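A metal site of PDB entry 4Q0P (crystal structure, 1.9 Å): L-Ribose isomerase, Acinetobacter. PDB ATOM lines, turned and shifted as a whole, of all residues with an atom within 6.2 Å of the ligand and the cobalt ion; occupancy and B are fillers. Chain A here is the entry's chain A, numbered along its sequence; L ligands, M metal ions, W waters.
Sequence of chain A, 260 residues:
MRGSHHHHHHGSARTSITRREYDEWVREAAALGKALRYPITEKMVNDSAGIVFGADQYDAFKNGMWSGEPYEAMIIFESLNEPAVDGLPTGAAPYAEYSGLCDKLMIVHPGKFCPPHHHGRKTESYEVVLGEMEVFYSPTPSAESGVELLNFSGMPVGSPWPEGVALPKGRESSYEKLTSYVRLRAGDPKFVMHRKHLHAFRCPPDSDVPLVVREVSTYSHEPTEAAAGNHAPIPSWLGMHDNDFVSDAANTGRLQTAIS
The cobalt ion is bound by OE2 of Glu 124 (2.1 Å), NE2 of His 199 (2.2 Å), water W1 (2.2 Å), NE2 of His 119 (2.2 Å), NE2 of His 117 (2.3 Å) and O5 of the ligand (2.4 Å).
The cobalt ion has six donor atoms within binding distance.
O2 of the ligand sits at hydrogen-bond distance from NZ of Lys 122.
The side-chain carboxylate (OE2) of Glu 222 sits at hydrogen-bond distance from an oxygen (O4) of the ligand (3.3 Å).
OD1 of Asn 243 is in hydrogen-bond range of O4 of the ligand (3.2 Å).
An oxygen (O1) of the ligand sits at hydrogen-bond distance from the side-chain sulfur of Met 106 (3.4 Å).
The side-chain carboxylate (OE2) of Glu 215 sits at hydrogen-bond distance from an oxygen (O2) of the ligand, 2.5 Å away.
Of the 23 residues printed, 4 come within 4 Å of the cobalt ion.
The nearest printed residue that does not touch the cobalt ion is Lys 122 (4.7 Å).
Ile 76 touches the ligand (CD1 to C3, 3.6 Å).
NZ of Lys 104 touches O2 of the ligand (3.8 Å).
Cys 114 touches the ligand.
Ser 220 touches the ligand (OG to O4, 3.9 Å).
NH1 of Arg 254 touches C4 of the ligand, at 3.9 Å.
Hydrophobic or aromatic side chains within 4 Å of the ligand: Ile 76, Met 106 and His 119.
Of the 23 residues printed, 13 come within 4 Å of the ligand.
The nearest printed residue that does not touch the ligand is Phe 201 (4.1 Å).
Water W1 lies within hydrogen-bond range of OE1 of Glu 124 (2.7 Å) and O1 of the ligand (2.8 Å).
Water W2 lies within hydrogen-bond range of OE1 of Glu 78 (2.8 Å), O3 of the ligand (2.9 Å) and SG of Cys 102 (3.5 Å).
OG of Ser 220 sits at hydrogen-bond distance from NZ of Lys 122 (3.1 Å).
The backbone NH (N) of Cys 114 lies within hydrogen-bond range of the backbone carbonyl oxygen (O) of Phe 201 (2.8 Å).
NZ of Lys 104 lies within hydrogen-bond range of OG of Ser 217, 2.9 Å away.
The side-chain hydroxyl (OH) of Tyr 126 lies within hydrogen-bond range of the side-chain carboxylate (OE1) of Glu 124 (2.7 Å).
The side-chain carboxylate (OE2) of Glu 222 is in salt-bridge range of the guanidinium group (NH1) of Arg 254, 2.6 Å away.
OE2 of Glu 215 lies within hydrogen-bond range of OG of Ser 217.
ND2 of Asn 243 sits at hydrogen-bond distance from OE2 of Glu 222 (2.5 Å).
The side-chain amide oxygen (OD1) of Asn 243 sits at hydrogen-bond distance from a ring nitrogen (ND1) of His 119, 2.9 Å away.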
ATOM      1  N   MET A  74     -13.003 -17.777 -12.667  1.00  0.00           N
ATOM      2  CA  MET A  74     -13.897 -17.390 -13.735  1.00  0.00           C
ATOM      3  C   MET A  74     -15.135 -16.729 -13.193  1.00  0.00           C
ATOM      4  O   MET A  74     -15.372 -16.712 -11.983  1.00  0.00           O
ATOM      5  CB  MET A  74     -14.330 -18.624 -14.537  1.00  0.00           C
ATOM      6  CG  MET A  74     -15.365 -19.462 -13.810  1.00  0.00           C
ATOM      7  SD  MET A  74     -15.633 -21.042 -14.622  1.00  0.00           S
ATOM      8  CE  MET A  74     -16.390 -20.503 -16.149  1.00  0.00           C
ATOM      9  N   ILE A  76     -19.398 -16.458 -13.785  1.00  0.00           N
ATOM     10  CA  ILE A  76     -20.545 -17.123 -14.371  1.00  0.00           C
ATOM     11  C   ILE A  76     -21.820 -16.362 -14.047  1.00  0.00           C
ATOM     12  O   ILE A  76     -22.093 -16.064 -12.874  1.00  0.00           O
ATOM     13  CB  ILE A  76     -20.706 -18.573 -13.860  1.00  0.00           C
ATOM     14  CG1 ILE A  76     -19.499 -19.416 -14.295  1.00  0.00           C
ATOM     15  CG2 ILE A  76     -22.008 -19.168 -14.379  1.00  0.00           C
ATOM     16  CD1 ILE A  76     -19.578 -20.883 -13.892  1.00  0.00           C
ATOM     17  N   GLU A  78     -25.666 -16.879 -14.518  1.00  0.00           N
ATOM     18  CA  GLU A  78     -26.675 -17.867 -14.845  1.00  0.00           C
ATOM     19  C   GLU A  78     -28.052 -17.262 -15.034  1.00  0.00           C
ATOM     20  O   GLU A  78     -28.625 -16.697 -14.089  1.00  0.00           O
ATOM     21  CB  GLU A  78     -26.696 -18.915 -13.728  1.00  0.00           C
ATOM     22  CG  GLU A  78     -27.747 -19.985 -13.831  1.00  0.00           C
ATOM     23  CD  GLU A  78     -27.728 -20.906 -12.629  1.00  0.00           C
ATOM     24  OE1 GLU A  78     -26.760 -21.697 -12.503  1.00  0.00           O
ATOM     25  OE2 GLU A  78     -28.666 -20.829 -11.802  1.00  0.00           O
ATOM     26  N   CYS A 102     -30.101 -25.428 -18.108  1.00  0.00           N
ATOM     27  CA  CYS A 102     -29.286 -24.406 -17.466  1.00  0.00           C
ATOM     28  C   CYS A 102     -28.573 -23.578 -18.543  1.00  0.00           C
ATOM     29  O   CYS A 102     -27.802 -24.116 -19.351  1.00  0.00           O
ATOM     30  CB  CYS A 102     -28.271 -25.058 -16.517  1.00  0.00           C
ATOM     31  SG  CYS A 102     -27.186 -23.903 -15.646  1.00  0.00           S
ATOM     32  N   LYS A 104     -26.165 -20.182 -19.124  1.00  0.00           N
ATOM     33  CA  LYS A 104     -25.308 -19.241 -18.422  1.00  0.00           C
ATOM     34  C   LYS A 104     -24.255 -18.675 -19.339  1.00  0.00           C
ATOM     35  O   LYS A 104     -23.917 -19.276 -20.367  1.00  0.00           O
ATOM     36  CB  LYS A 104     -24.615 -19.919 -17.239  1.00  0.00           C
ATOM     37  CG  LYS A 104     -23.495 -20.883 -17.650  1.00  0.00           C
ATOM     38  CD  LYS A 104     -23.755 -22.307 -17.132  1.00  0.00           C
ATOM     39  CE  LYS A 104     -24.945 -22.949 -17.828  1.00  0.00           C
ATOM     40  NZ  LYS A 104     -25.129 -24.376 -17.418  1.00  0.00           N
ATOM     41  N   MET A 106     -20.335 -17.448 -19.381  1.00  0.00           N
ATOM     42  CA  MET A 106     -19.117 -17.618 -18.584  1.00  0.00           C
ATOM     43  C   MET A 106     -18.020 -16.726 -19.139  1.00  0.00           C
ATOM     44  O   MET A 106     -17.834 -16.648 -20.354  1.00  0.00           O
ATOM     45  CB  MET A 106     -18.685 -19.095 -18.588  1.00  0.00           C
ATOM     46  CG  MET A 106     -19.749 -20.049 -18.045  1.00  0.00           C
ATOM     47  SD  MET A 106     -19.282 -21.808 -18.012  1.00  0.00           S
ATOM     48  CE  MET A 106     -18.830 -22.054 -19.733  1.00  0.00           C
ATOM     49  N   CYS A 114     -11.064 -22.776 -16.265  1.00  0.00           N
ATOM     50  CA  CYS A 114     -12.223 -23.324 -15.574  1.00  0.00           C
ATOM     51  C   CYS A 114     -11.495 -24.667 -15.433  1.00  0.00           C
ATOM     52  O   CYS A 114     -11.321 -25.392 -16.429  1.00  0.00           O
ATOM     53  CB  CYS A 114     -13.433 -23.480 -16.483  1.00  0.00           C
ATOM     54  SG  CYS A 114     -14.783 -24.407 -15.681  1.00  0.00           S
ATOM     55  N   HIS A 117     -12.529 -31.054 -14.314  1.00  0.00           N
ATOM     56  CA  HIS A 117     -13.636 -31.562 -13.518  1.00  0.00           C
ATOM     57  C   HIS A 117     -14.575 -32.376 -14.409  1.00  0.00           C
ATOM     58  O   HIS A 117     -14.406 -32.408 -15.628  1.00  0.00           O
ATOM     59  CB  HIS A 117     -14.413 -30.400 -12.908  1.00  0.00           C
ATOM     60  CG  HIS A 117     -15.137 -29.550 -13.909  1.00  0.00           C
ATOM     61  ND1 HIS A 117     -14.490 -28.662 -14.746  1.00  0.00           N
ATOM     62  CD2 HIS A 117     -16.447 -29.488 -14.240  1.00  0.00           C
ATOM     63  CE1 HIS A 117     -15.371 -28.081 -15.543  1.00  0.00           C
ATOM     64  NE2 HIS A 117     -16.567 -28.568 -15.264  1.00  0.00           N
ATOM     65  N   HIS A 118     -15.545 -33.020 -13.791  1.00  0.00           N
ATOM     66  CA  HIS A 118     -16.537 -33.771 -14.553  1.00  0.00           C
ATOM     67  C   HIS A 118     -17.844 -33.799 -13.783  1.00  0.00           C
ATOM     68  O   HIS A 118     -17.885 -33.513 -12.592  1.00  0.00           O
ATOM     69  CB  HIS A 118     -16.040 -35.206 -14.854  1.00  0.00           C
ATOM     70  CG  HIS A 118     -16.272 -36.189 -13.755  1.00  0.00           C
ATOM     71  ND1 HIS A 118     -15.429 -36.295 -12.662  1.00  0.00           N
ATOM     72  CD2 HIS A 118     -17.231 -37.120 -13.574  1.00  0.00           C
ATOM     73  CE1 HIS A 118     -15.874 -37.246 -11.865  1.00  0.00           C
ATOM     74  NE2 HIS A 118     -16.963 -37.769 -12.393  1.00  0.00           N
ATOM     75  N   HIS A 119     -18.917 -34.118 -14.487  1.00  0.00           N
ATOM     76  CA  HIS A 119     -20.233 -34.175 -13.869  1.00  0.00           C
ATOM     77  C   HIS A 119     -20.809 -35.552 -14.146  1.00  0.00           C
ATOM     78  O   HIS A 119     -20.628 -36.112 -15.228  1.00  0.00           O
ATOM     79  CB  HIS A 119     -21.155 -33.126 -14.493  1.00  0.00           C
ATOM     80  CG  HIS A 119     -20.518 -31.782 -14.635  1.00  0.00           C
ATOM     81  ND1 HIS A 119     -20.257 -30.961 -13.553  1.00  0.00           N
ATOM     82  CD2 HIS A 119     -20.066 -31.122 -15.726  1.00  0.00           C
ATOM     83  CE1 HIS A 119     -19.667 -29.852 -13.983  1.00  0.00           C
ATOM     84  NE2 HIS A 119     -19.534 -29.934 -15.292  1.00  0.00           N
ATOM     85  N   LYS A 122     -24.729 -33.744 -15.427  1.00  0.00           N
ATOM     86  CA  LYS A 122     -24.772 -32.653 -16.390  1.00  0.00           C
ATOM     87  C   LYS A 122     -24.004 -32.791 -17.698  1.00  0.00           C
ATOM     88  O   LYS A 122     -22.795 -33.050 -17.711  1.00  0.00           O
ATOM     89  CB  LYS A 122     -24.331 -31.349 -15.708  1.00  0.00           C
ATOM     90  CG  LYS A 122     -24.440 -30.121 -16.595  1.00  0.00           C
ATOM     91  CD  LYS A 122     -24.272 -28.842 -15.792  1.00  0.00           C
ATOM     92  CE  LYS A 122     -22.879 -28.744 -15.213  1.00  0.00           C
ATOM     93  NZ  LYS A 122     -22.755 -27.577 -14.306  1.00  0.00           N
ATOM     94  N   GLU A 124     -23.130 -30.643 -21.094  1.00  0.00           N
ATOM     95  CA  GLU A 124     -23.042 -29.240 -21.504  1.00  0.00           C
ATOM     96  C   GLU A 124     -22.803 -29.064 -23.004  1.00  0.00           C
ATOM     97  O   GLU A 124     -22.455 -29.998 -23.713  1.00  0.00           O
ATOM     98  CB  GLU A 124     -21.879 -28.550 -20.771  1.00  0.00           C
ATOM     99  CG  GLU A 124     -21.623 -29.047 -19.357  1.00  0.00           C
ATOM    100  CD  GLU A 124     -20.319 -28.517 -18.751  1.00  0.00           C
ATOM    101  OE1 GLU A 124     -19.356 -28.210 -19.491  1.00  0.00           O
ATOM    102  OE2 GLU A 124     -20.254 -28.416 -17.505  1.00  0.00           O
ATOM    103  N   TYR A 126     -21.242 -25.746 -25.726  1.00  0.00           N
ATOM    104  CA  TYR A 126     -20.618 -24.437 -25.750  1.00  0.00           C
ATOM    105  C   TYR A 126     -20.840 -23.667 -27.038  1.00  0.00           C
ATOM    106  O   TYR A 126     -20.837 -24.241 -28.135  1.00  0.00           O
ATOM    107  CB  TYR A 126     -19.094 -24.537 -25.548  1.00  0.00           C
ATOM    108  CG  TYR A 126     -18.665 -25.456 -24.439  1.00  0.00           C
ATOM    109  CD1 TYR A 126     -19.203 -25.351 -23.158  1.00  0.00           C
ATOM    110  CD2 TYR A 126     -17.727 -26.456 -24.682  1.00  0.00           C
ATOM    111  CE1 TYR A 126     -18.823 -26.228 -22.147  1.00  0.00           C
ATOM    112  CE2 TYR A 126     -17.340 -27.337 -23.675  1.00  0.00           C
ATOM    113  CZ  TYR A 126     -17.887 -27.226 -22.414  1.00  0.00           C
ATOM    114  OH  TYR A 126     -17.523 -28.112 -21.439  1.00  0.00           O
ATOM    115  N   MET A 193     -20.275 -31.407 -24.547  1.00  0.00           N
ATOM    116  CA  MET A 193     -19.418 -32.076 -23.577  1.00  0.00           C
ATOM    117  C   MET A 193     -20.345 -33.008 -22.800  1.00  0.00           C
ATOM    118  O   MET A 193     -21.063 -32.579 -21.886  1.00  0.00           O
ATOM    119  CB  MET A 193     -18.761 -31.069 -22.623  1.00  0.00           C
ATOM    120  CG  MET A 193     -17.794 -31.697 -21.605  1.00  0.00           C
ATOM    121  SD  MET A 193     -16.416 -32.655 -22.374  1.00  0.00           S
ATOM    122  CE  MET A 193     -15.581 -31.377 -23.297  1.00  0.00           C
ATOM    123  N   HIS A 199     -13.223 -32.517 -18.162  1.00  0.00           N
ATOM    124  CA  HIS A 199     -13.027 -31.381 -19.047  1.00  0.00           C
ATOM    125  C   HIS A 199     -12.558 -30.138 -18.324  1.00  0.00           C
ATOM    126  O   HIS A 199     -12.727 -29.994 -17.112  1.00  0.00           O
ATOM    127  CB  HIS A 199     -14.302 -31.081 -19.851  1.00  0.00           C
ATOM    128  CG  HIS A 199     -15.512 -30.789 -19.009  1.00  0.00           C
ATOM    129  ND1 HIS A 199     -16.149 -31.756 -18.267  1.00  0.00           N
ATOM    130  CD2 HIS A 199     -16.191 -29.641 -18.799  1.00  0.00           C
ATOM    131  CE1 HIS A 199     -17.178 -31.218 -17.633  1.00  0.00           C
ATOM    132  NE2 HIS A 199     -17.225 -29.942 -17.943  1.00  0.00           N
ATOM    133  N   PHE A 201     -11.130 -25.778 -19.558  1.00  0.00           N
ATOM    134  CA  PHE A 201     -10.963 -24.854 -20.660  1.00  0.00           C
ATOM    135  C   PHE A 201     -10.351 -23.538 -20.184  1.00  0.00           C
ATOM    136  O   PHE A 201     -10.443 -23.194 -19.003  1.00  0.00           O
ATOM    137  CB  PHE A 201     -12.284 -24.625 -21.404  1.00  0.00           C
ATOM    138  CG  PHE A 201     -13.393 -24.038 -20.566  1.00  0.00           C
ATOM    139  CD1 PHE A 201     -13.510 -22.662 -20.389  1.00  0.00           C
ATOM    140  CD2 PHE A 201     -14.350 -24.870 -19.975  1.00  0.00           C
ATOM    141  CE1 PHE A 201     -14.567 -22.117 -19.658  1.00  0.00           C
ATOM    142  CE2 PHE A 201     -15.404 -24.333 -19.232  1.00  0.00           C
ATOM    143  CZ  PHE A 201     -15.516 -22.954 -19.072  1.00  0.00           C
ATOM    144  N   GLU A 215     -23.117 -21.220 -22.217  1.00  0.00           N
ATOM    145  CA  GLU A 215     -23.261 -22.643 -22.000  1.00  0.00           C
ATOM    146  C   GLU A 215     -24.728 -23.011 -21.844  1.00  0.00           C
ATOM    147  O   GLU A 215     -25.469 -22.370 -21.090  1.00  0.00           O
ATOM    148  CB  GLU A 215     -22.515 -23.092 -20.747  1.00  0.00           C
ATOM    149  CG  GLU A 215     -22.773 -24.562 -20.412  1.00  0.00           C
ATOM    150  CD  GLU A 215     -22.072 -25.004 -19.152  1.00  0.00           C
ATOM    151  OE1 GLU A 215     -20.815 -24.987 -19.150  1.00  0.00           O
ATOM    152  OE2 GLU A 215     -22.754 -25.360 -18.172  1.00  0.00           O
ATOM    153  N   SER A 217     -26.747 -26.324 -20.901  1.00  0.00           N
ATOM    154  CA  SER A 217     -26.571 -27.668 -20.384  1.00  0.00           C
ATOM    155  C   SER A 217     -27.814 -28.122 -19.622  1.00  0.00           C
ATOM    156  O   SER A 217     -28.788 -27.372 -19.509  1.00  0.00           O
ATOM    157  CB  SER A 217     -25.383 -27.709 -19.423  1.00  0.00           C
ATOM    158  OG  SER A 217     -25.722 -27.100 -18.194  1.00  0.00           O
ATOM    159  N   SER A 220     -27.989 -27.819 -13.358  1.00  0.00           N
ATOM    160  CA  SER A 220     -26.720 -27.718 -12.660  1.00  0.00           C
ATOM    161  C   SER A 220     -26.946 -27.860 -11.152  1.00  0.00           C
ATOM    162  O   SER A 220     -27.409 -26.933 -10.493  1.00  0.00           O
ATOM    163  CB  SER A 220     -26.050 -26.381 -12.976  1.00  0.00           C
ATOM    164  OG  SER A 220     -24.775 -26.289 -12.345  1.00  0.00           O
ATOM    165  N   GLU A 222     -25.883 -27.613  -7.724  1.00  0.00           N
ATOM    166  CA  GLU A 222     -24.849 -26.953  -6.953  1.00  0.00           C
ATOM    167  C   GLU A 222     -25.374 -26.360  -5.645  1.00  0.00           C
ATOM    168  O   GLU A 222     -25.995 -25.298  -5.638  1.00  0.00           O
ATOM    169  CB  GLU A 222     -24.205 -25.835  -7.790  1.00  0.00           C
ATOM    170  CG  GLU A 222     -23.551 -26.321  -9.064  1.00  0.00           C
ATOM    171  CD  GLU A 222     -23.016 -25.192  -9.936  1.00  0.00           C
ATOM    172  OE1 GLU A 222     -23.844 -24.416 -10.480  1.00  0.00           O
ATOM    173  OE2 GLU A 222     -21.786 -25.077 -10.070  1.00  0.00           O
ATOM    174  N   ASN A 243     -20.630 -31.362  -9.437  1.00  0.00           N
ATOM    175  CA  ASN A 243     -19.412 -30.774  -9.990  1.00  0.00           C
ATOM    176  C   ASN A 243     -18.214 -31.400  -9.283  1.00  0.00           C
ATOM    177  O   ASN A 243     -17.838 -30.991  -8.187  1.00  0.00           O
ATOM    178  CB  ASN A 243     -19.393 -29.256  -9.801  1.00  0.00           C
ATOM    179  CG  ASN A 243     -20.549 -28.551 -10.477  1.00  0.00           C
ATOM    180  OD1 ASN A 243     -21.037 -29.001 -11.520  1.00  0.00           O
ATOM    181  ND2 ASN A 243     -20.983 -27.450  -9.898  1.00  0.00           N
ATOM    182  N   PHE A 245     -14.414 -31.801  -9.165  1.00  0.00           N
ATOM    183  CA  PHE A 245     -13.143 -31.269  -9.622  1.00  0.00           C
ATOM    184  C   PHE A 245     -12.008 -32.247  -9.322  1.00  0.00           C
ATOM    185  O   PHE A 245     -11.978 -32.855  -8.261  1.00  0.00           O
ATOM    186  CB  PHE A 245     -12.888 -29.905  -8.975  1.00  0.00           C
ATOM    187  CG  PHE A 245     -13.767 -28.817  -9.526  1.00  0.00           C
ATOM    188  CD1 PHE A 245     -13.434 -28.139 -10.695  1.00  0.00           C
ATOM    189  CD2 PHE A 245     -14.975 -28.503  -8.892  1.00  0.00           C
ATOM    190  CE1 PHE A 245     -14.285 -27.183 -11.241  1.00  0.00           C
ATOM    191  CE2 PHE A 245     -15.834 -27.543  -9.434  1.00  0.00           C
ATOM    192  CZ  PHE A 245     -15.489 -26.883 -10.608  1.00  0.00           C
ATOM    193  N   ARG A 254     -14.784 -23.354  -4.153  1.00  0.00           N
ATOM    194  CA  ARG A 254     -15.673 -23.096  -5.276  1.00  0.00           C
ATOM    195  C   ARG A 254     -17.034 -22.584  -4.804  1.00  0.00           C
ATOM    196  O   ARG A 254     -17.648 -21.729  -5.447  1.00  0.00           O
ATOM    197  CB  ARG A 254     -15.845 -24.383  -6.100  1.00  0.00           C
ATOM    198  CG  ARG A 254     -16.441 -24.195  -7.493  1.00  0.00           C
ATOM    199  CD  ARG A 254     -17.916 -23.833  -7.452  1.00  0.00           C
ATOM    200  NE  ARG A 254     -18.466 -23.649  -8.791  1.00  0.00           N
ATOM    201  CZ  ARG A 254     -19.713 -23.272  -9.036  1.00  0.00           C
ATOM    202  NH1 ARG A 254     -20.119 -23.127 -10.299  1.00  0.00           N
ATOM    203  NH2 ARG A 254     -20.551 -23.017  -8.037  1.00  0.00           N
HETATM  204  C1  LIG L   1     -19.568 -25.676 -16.410  1.00  0.00           C
HETATM  205  C2  LIG L   1     -20.794 -24.927 -15.893  1.00  0.00           C
HETATM  206  C3  LIG L   1     -20.531 -24.329 -14.507  1.00  0.00           C
HETATM  207  C4  LIG L   1     -19.915 -25.348 -13.532  1.00  0.00           C
HETATM  208  C5  LIG L   1     -18.757 -26.126 -14.170  1.00  0.00           C
HETATM  209  O1  LIG L   1     -18.492 -24.766 -16.574  1.00  0.00           O
HETATM  210  O2  LIG L   1     -21.913 -25.798 -15.855  1.00  0.00           O
HETATM  211  O3  LIG L   1     -21.751 -23.848 -13.971  1.00  0.00           O
HETATM  212  O4  LIG L   1     -20.912 -26.259 -13.074  1.00  0.00           O
HETATM  213  O5  LIG L   1     -19.155 -26.673 -15.439  1.00  0.00           O
HETATM  214 CO    CO M   1     -18.372 -28.645 -16.638  1.00  0.00          CO
HETATM  215  O   HOH W   1     -17.475 -27.064 -17.864  1.00  0.00           O
HETATM  216  O   HOH W   2     -24.481 -22.766 -13.764  1.00  0.00           O
